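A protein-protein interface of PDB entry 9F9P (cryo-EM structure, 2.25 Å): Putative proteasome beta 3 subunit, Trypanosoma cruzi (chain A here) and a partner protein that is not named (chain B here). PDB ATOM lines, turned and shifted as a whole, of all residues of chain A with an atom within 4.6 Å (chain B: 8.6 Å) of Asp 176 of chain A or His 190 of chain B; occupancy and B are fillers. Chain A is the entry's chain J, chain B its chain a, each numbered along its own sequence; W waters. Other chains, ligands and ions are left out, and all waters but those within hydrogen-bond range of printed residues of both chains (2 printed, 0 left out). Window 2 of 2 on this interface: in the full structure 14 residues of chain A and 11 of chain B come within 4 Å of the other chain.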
ATOM      1  N   GLN A 169      13.761  -7.877 -11.652  1.00  0.00           N
ATOM      2  CA  GLN A 169      15.093  -7.466 -12.064  1.00  0.00           C
ATOM      3  C   GLN A 169      15.312  -7.675 -13.565  1.00  0.00           C
ATOM      4  O   GLN A 169      16.051  -6.916 -14.189  1.00  0.00           O
ATOM      5  CB  GLN A 169      16.184  -8.222 -11.296  1.00  0.00           C
ATOM      6  CG  GLN A 169      16.303  -7.790  -9.844  1.00  0.00           C
ATOM      7  CD  GLN A 169      16.566  -6.303  -9.651  1.00  0.00           C
ATOM      8  OE1 GLN A 169      17.512  -5.722 -10.192  1.00  0.00           O
ATOM      9  NE2 GLN A 169      15.710  -5.654  -8.876  1.00  0.00           N
ATOM     10  N   LEU A 172      13.386  -4.733 -15.348  1.00  0.00           N
ATOM     11  CA  LEU A 172      13.998  -3.411 -15.186  1.00  0.00           C
ATOM     12  C   LEU A 172      15.360  -3.276 -15.872  1.00  0.00           C
ATOM     13  O   LEU A 172      15.673  -2.213 -16.392  1.00  0.00           O
ATOM     14  CB  LEU A 172      14.174  -3.098 -13.701  1.00  0.00           C
ATOM     15  CG  LEU A 172      12.852  -2.967 -12.952  1.00  0.00           C
ATOM     16  CD1 LEU A 172      13.064  -2.742 -11.470  1.00  0.00           C
ATOM     17  CD2 LEU A 172      11.982  -1.859 -13.548  1.00  0.00           C
ATOM     18  N   SER A 173      16.188  -4.312 -15.868  1.00  0.00           N
ATOM     19  CA  SER A 173      17.449  -4.215 -16.570  1.00  0.00           C
ATOM     20  C   SER A 173      17.251  -4.110 -18.076  1.00  0.00           C
ATOM     21  O   SER A 173      17.962  -3.377 -18.746  1.00  0.00           O
ATOM     22  CB  SER A 173      18.328  -5.382 -16.250  1.00  0.00           C
ATOM     23  OG  SER A 173      18.386  -5.522 -14.848  1.00  0.00           O
ATOM     24  N   ALA A 174      16.286  -4.824 -18.624  1.00  0.00           N
ATOM     25  CA  ALA A 174      16.110  -4.785 -20.063  1.00  0.00           C
ATOM     26  C   ALA A 174      15.510  -3.469 -20.520  1.00  0.00           C
ATOM     27  O   ALA A 174      15.921  -2.943 -21.527  1.00  0.00           O
ATOM     28  CB  ALA A 174      15.234  -5.921 -20.475  1.00  0.00           C
ATOM     29  N   CYS A 175      14.525  -2.962 -19.793  1.00  0.00           N
ATOM     30  CA  CYS A 175      13.916  -1.686 -20.101  1.00  0.00           C
ATOM     31  C   CYS A 175      14.916  -0.528 -20.027  1.00  0.00           C
ATOM     32  O   CYS A 175      14.807   0.393 -20.829  1.00  0.00           O
ATOM     33  CB  CYS A 175      12.732  -1.408 -19.176  1.00  0.00           C
ATOM     34  SG  CYS A 175      11.276  -2.406 -19.613  1.00  0.00           S
ATOM     35  N   ASP A 176      15.897  -0.571 -19.116  1.00  0.00           N
ATOM     36  CA  ASP A 176      16.911   0.467 -19.082  1.00  0.00           C
ATOM     37  C   ASP A 176      17.819   0.477 -20.313  1.00  0.00           C
ATOM     38  O   ASP A 176      18.385   1.517 -20.606  1.00  0.00           O
ATOM     39  CB  ASP A 176      17.724   0.422 -17.801  1.00  0.00           C
ATOM     40  CG  ASP A 176      16.880   0.709 -16.559  1.00  0.00           C
ATOM     41  OD1 ASP A 176      15.687   1.095 -16.698  1.00  0.00           O
ATOM     42  OD2 ASP A 176      17.414   0.505 -15.441  1.00  0.00           O
ATOM     43  N   ARG A 177      17.885  -0.571 -21.107  1.00  0.00           N
ATOM     44  CA  ARG A 177      18.609  -0.456 -22.347  1.00  0.00           C
ATOM     45  C   ARG A 177      17.674  -0.217 -23.540  1.00  0.00           C
ATOM     46  O   ARG A 177      18.138  -0.296 -24.661  1.00  0.00           O
ATOM     47  CB  ARG A 177      19.458  -1.713 -22.591  1.00  0.00           C
ATOM     48  CG  ARG A 177      20.711  -1.838 -21.724  1.00  0.00           C
ATOM     49  CD  ARG A 177      21.842  -0.928 -22.196  1.00  0.00           C
ATOM     50  NE  ARG A 177      22.995  -0.914 -21.309  1.00  0.00           N
ATOM     51  CZ  ARG A 177      24.069  -0.128 -21.442  1.00  0.00           C
ATOM     52  NH1 ARG A 177      24.231   0.649 -22.501  1.00  0.00           N
ATOM     53  NH2 ARG A 177      25.004  -0.139 -20.504  1.00  0.00           N
ATOM     54  N   ASP A 178      16.386   0.131 -23.324  1.00  0.00           N
ATOM     55  CA  ASP A 178      15.442   0.308 -24.432  1.00  0.00           C
ATOM     56  C   ASP A 178      14.739   1.665 -24.395  1.00  0.00           C
ATOM     57  O   ASP A 178      14.095   2.002 -23.413  1.00  0.00           O
ATOM     58  CB  ASP A 178      14.363  -0.791 -24.410  1.00  0.00           C
ATOM     59  CG  ASP A 178      13.489  -0.825 -25.670  1.00  0.00           C
ATOM     60  OD1 ASP A 178      14.049  -0.773 -26.794  1.00  0.00           O
ATOM     61  OD2 ASP A 178      12.250  -0.923 -25.541  1.00  0.00           O
ATOM     62  N   ARG A 203      12.790   3.798 -13.539  1.00  0.00           N
ATOM     63  CA  ARG A 203      13.292   5.081 -14.006  1.00  0.00           C
ATOM     64  C   ARG A 203      12.186   5.892 -14.676  1.00  0.00           C
ATOM     65  O   ARG A 203      11.183   5.343 -15.097  1.00  0.00           O
ATOM     66  CB  ARG A 203      14.431   4.840 -15.008  1.00  0.00           C
ATOM     67  CG  ARG A 203      15.765   4.425 -14.394  1.00  0.00           C
ATOM     68  CD  ARG A 203      16.886   4.551 -15.414  1.00  0.00           C
ATOM     69  NE  ARG A 203      17.281   5.921 -15.765  1.00  0.00           N
ATOM     70  CZ  ARG A 203      17.934   6.751 -14.951  1.00  0.00           C
ATOM     71  NH1 ARG A 203      18.454   6.294 -13.826  1.00  0.00           N
ATOM     72  NH2 ARG A 203      18.097   8.030 -15.277  1.00  0.00           N
ATOM     73  N   PRO B 180      23.059  -5.833 -20.537  1.00  0.00           N
ATOM     74  CA  PRO B 180      22.139  -5.661 -19.414  1.00  0.00           C
ATOM     75  C   PRO B 180      22.451  -6.515 -18.187  1.00  0.00           C
ATOM     76  O   PRO B 180      22.188  -6.079 -17.077  1.00  0.00           O
ATOM     77  CB  PRO B 180      20.729  -5.980 -19.934  1.00  0.00           C
ATOM     78  CG  PRO B 180      20.908  -6.460 -21.371  1.00  0.00           C
ATOM     79  CD  PRO B 180      22.338  -6.157 -21.774  1.00  0.00           C
ATOM     80  N   ASP B 183      25.256  -4.591 -16.379  1.00  0.00           N
ATOM     81  CA  ASP B 183      24.642  -3.471 -15.684  1.00  0.00           C
ATOM     82  C   ASP B 183      24.046  -3.943 -14.358  1.00  0.00           C
ATOM     83  O   ASP B 183      24.170  -3.247 -13.366  1.00  0.00           O
ATOM     84  CB  ASP B 183      23.525  -2.811 -16.500  1.00  0.00           C
ATOM     85  CG  ASP B 183      23.923  -2.117 -17.802  1.00  0.00           C
ATOM     86  OD1 ASP B 183      25.095  -1.703 -17.923  1.00  0.00           O
ATOM     87  OD2 ASP B 183      23.056  -2.002 -18.703  1.00  0.00           O
ATOM     88  N   CYS B 184      23.356  -5.086 -14.358  1.00  0.00           N
ATOM     89  CA  CYS B 184      22.639  -5.591 -13.192  1.00  0.00           C
ATOM     90  C   CYS B 184      23.657  -5.951 -12.107  1.00  0.00           C
ATOM     91  O   CYS B 184      23.616  -5.344 -11.045  1.00  0.00           O
ATOM     92  CB  CYS B 184      21.687  -6.769 -13.509  1.00  0.00           C
ATOM     93  SG  CYS B 184      20.579  -7.291 -12.147  1.00  0.00           S
ATOM     94  N   THR B 187      26.606  -2.611 -11.244  1.00  0.00           N
ATOM     95  CA  THR B 187      26.244  -1.256 -10.827  1.00  0.00           C
ATOM     96  C   THR B 187      25.075  -1.231  -9.825  1.00  0.00           C
ATOM     97  O   THR B 187      24.988  -0.318  -9.003  1.00  0.00           O
ATOM     98  CB  THR B 187      25.888  -0.383 -12.039  1.00  0.00           C
ATOM     99  OG1 THR B 187      24.559  -0.712 -12.454  1.00  0.00           O
ATOM    100  CG2 THR B 187      26.856  -0.528 -13.198  1.00  0.00           C
ATOM    101  N   ARG B 188      24.127  -2.175  -9.988  1.00  0.00           N
ATOM    102  CA  ARG B 188      23.074  -2.519  -9.034  1.00  0.00           C
ATOM    103  C   ARG B 188      22.168  -1.327  -8.702  1.00  0.00           C
ATOM    104  O   ARG B 188      21.915  -1.066  -7.524  1.00  0.00           O
ATOM    105  CB  ARG B 188      23.677  -3.056  -7.727  1.00  0.00           C
ATOM    106  CG  ARG B 188      24.797  -4.076  -7.893  1.00  0.00           C
ATOM    107  CD  ARG B 188      25.438  -4.439  -6.562  1.00  0.00           C
ATOM    108  NE  ARG B 188      24.748  -5.517  -5.865  1.00  0.00           N
ATOM    109  CZ  ARG B 188      25.092  -5.979  -4.667  1.00  0.00           C
ATOM    110  NH1 ARG B 188      24.499  -7.054  -4.183  1.00  0.00           N
ATOM    111  NH2 ARG B 188      26.051  -5.388  -3.972  1.00  0.00           N
ATOM    112  N   GLN B 189      21.623  -0.647  -9.725  1.00  0.00           N
ATOM    113  CA  GLN B 189      20.870   0.584  -9.498  1.00  0.00           C
ATOM    114  C   GLN B 189      19.405   0.288  -9.143  1.00  0.00           C
ATOM    115  O   GLN B 189      18.654   1.226  -8.859  1.00  0.00           O
ATOM    116  CB  GLN B 189      20.980   1.558 -10.688  1.00  0.00           C
ATOM    117  CG  GLN B 189      19.977   1.331 -11.824  1.00  0.00           C
ATOM    118  CD  GLN B 189      19.600   2.567 -12.622  1.00  0.00           C
ATOM    119  OE1 GLN B 189      19.021   3.531 -12.113  1.00  0.00           O
ATOM    120  NE2 GLN B 189      19.877   2.523 -13.918  1.00  0.00           N
ATOM    121  N   HIS B 190      18.993  -0.997  -9.136  1.00  0.00           N
ATOM    122  CA  HIS B 190      17.595  -1.370  -8.900  1.00  0.00           C
ATOM    123  C   HIS B 190      17.419  -2.205  -7.619  1.00  0.00           C
ATOM    124  O   HIS B 190      16.383  -2.852  -7.453  1.00  0.00           O
ATOM    125  CB  HIS B 190      17.013  -2.074 -10.145  1.00  0.00           C
ATOM    126  CG  HIS B 190      16.719  -1.162 -11.300  1.00  0.00           C
ATOM    127  ND1 HIS B 190      15.908  -0.044 -11.171  1.00  0.00           N
ATOM    128  CD2 HIS B 190      17.140  -1.175 -12.581  1.00  0.00           C
ATOM    129  CE1 HIS B 190      15.840   0.596 -12.334  1.00  0.00           C
ATOM    130  NE2 HIS B 190      16.577  -0.076 -13.206  1.00  0.00           N
ATOM    131  N   MET B 191      18.392  -2.147  -6.685  1.00  0.00           N
ATOM    132  CA  MET B 191      18.508  -3.135  -5.611  1.00  0.00           C
ATOM    133  C   MET B 191      18.477  -2.481  -4.214  1.00  0.00           C
ATOM    134  O   MET B 191      18.543  -1.240  -4.135  1.00  0.00           O
ATOM    135  CB  MET B 191      19.791  -3.967  -5.788  1.00  0.00           C
ATOM    136  CG  MET B 191      19.701  -4.949  -6.977  1.00  0.00           C
ATOM    137  SD  MET B 191      21.055  -6.147  -7.155  1.00  0.00           S
ATOM    138  CE  MET B 191      21.006  -6.430  -8.927  1.00  0.00           C
HETATM  139  O   HOH W   1      20.364  -2.105 -17.953  1.00  0.00           O
HETATM  140  O   HOH W   2      13.738   0.998 -14.937  1.00  0.00           O
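The side-chain hydroxyl (OG1) of Thr 187 of chain B is in hydrogen-bond range of the backbone carbonyl oxygen (O) of Asp 183 of chain B (2.7 Å).
The side-chain hydroxyl (OG) of Ser 173 of chain A lies within hydrogen-bond range of the backbone carbonyl oxygen (O) of Gln 169 of chain A, 2.8 Å away.
Water W2 lies within hydrogen-bond range of OD1 of Asp 176 of chain A, N of Arg 203 of chain A and NE2 of His 190 of chain B.
Water W1 bridges the side-chain carboxylate (OD2) of Asp 183 of chain B (2.8 Å) and the backbone carbonyl oxygen (O) of Ser 173 of chain A (2.8 Å).
Hydrophobic or aromatic side chains of chain B that line the printed part of chain A: Pro 180, His 190 and Met 191.
Among the printed residues, 10 pairs touch across the chains.
Among the printed residues, Asp or Glu carboxylates within 4 Å of a Lys or Arg side-chain nitrogen of the other chain: Arg 177 of chain A with Asp 183 of chain B (2.8 Å).
Among the printed residues, pairs that only touch across the chains: Gln 169 of chain A with Cys 184 of chain B (3.96 Å), Gln 169 of chain A with Met 191 of chain B (3.8 Å), Leu 172 of chain A with His 190 of chain B (3.7 Å), Ser 173 of chain A with Pro 180 of chain B (3.98 Å), Ser 173 of chain A with Cys 184 of chain B (3.8 Å) and Asp 176 of chain A with Gln 189 of chain B (3.5 Å).
Asp 176 of chain A touches just these residues of chain B: Gln 189 and His 190.
His 190 of chain B touches just these residues of chain A: Gln 169, Leu 172 and Asp 176.
Of the printed residues of chain A, Met 191 of chain B touches Gln 169.
Printed residues of chain A within 4 Å of Pro 180 of chain B: Ser 173 (3.98 Å).
Thr 187 of chain B touches none of the printed residues of chain A.
The nearest residue of chain B that does not touch Asp 176 of chain A is Asp 183 of chain B (5.9 Å).
The nearest residue of chain A that does not touch His 190 of chain B is Arg 203 of chain A (4.3 Å).
The nearest printed residue of chain B that does not touch Leu 172 of chain A is Gln 189 of chain B (6.8 Å).
The side-chain amide nitrogen (NE2) of Gln 169 of chain A sits at hydrogen-bond distance from the backbone carbonyl oxygen (O) of His 190 of chain B (3.2 Å).
The guanidinium group (NE) of Arg 177 of chain A lies within salt-bridge range of the side-chain carboxylate (OD2) of Asp 183 of chain B (2.8 Å).
The side-chain amide oxygen of Gln 189 of chain B lies within hydrogen-bond range of the guanidinium group of Arg 203 of chain A (3.3 Å).
OD2 of Asp 176 of chain A sits at hydrogen-bond distance from NE2 of His 190 of chain B (2.5 Å).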
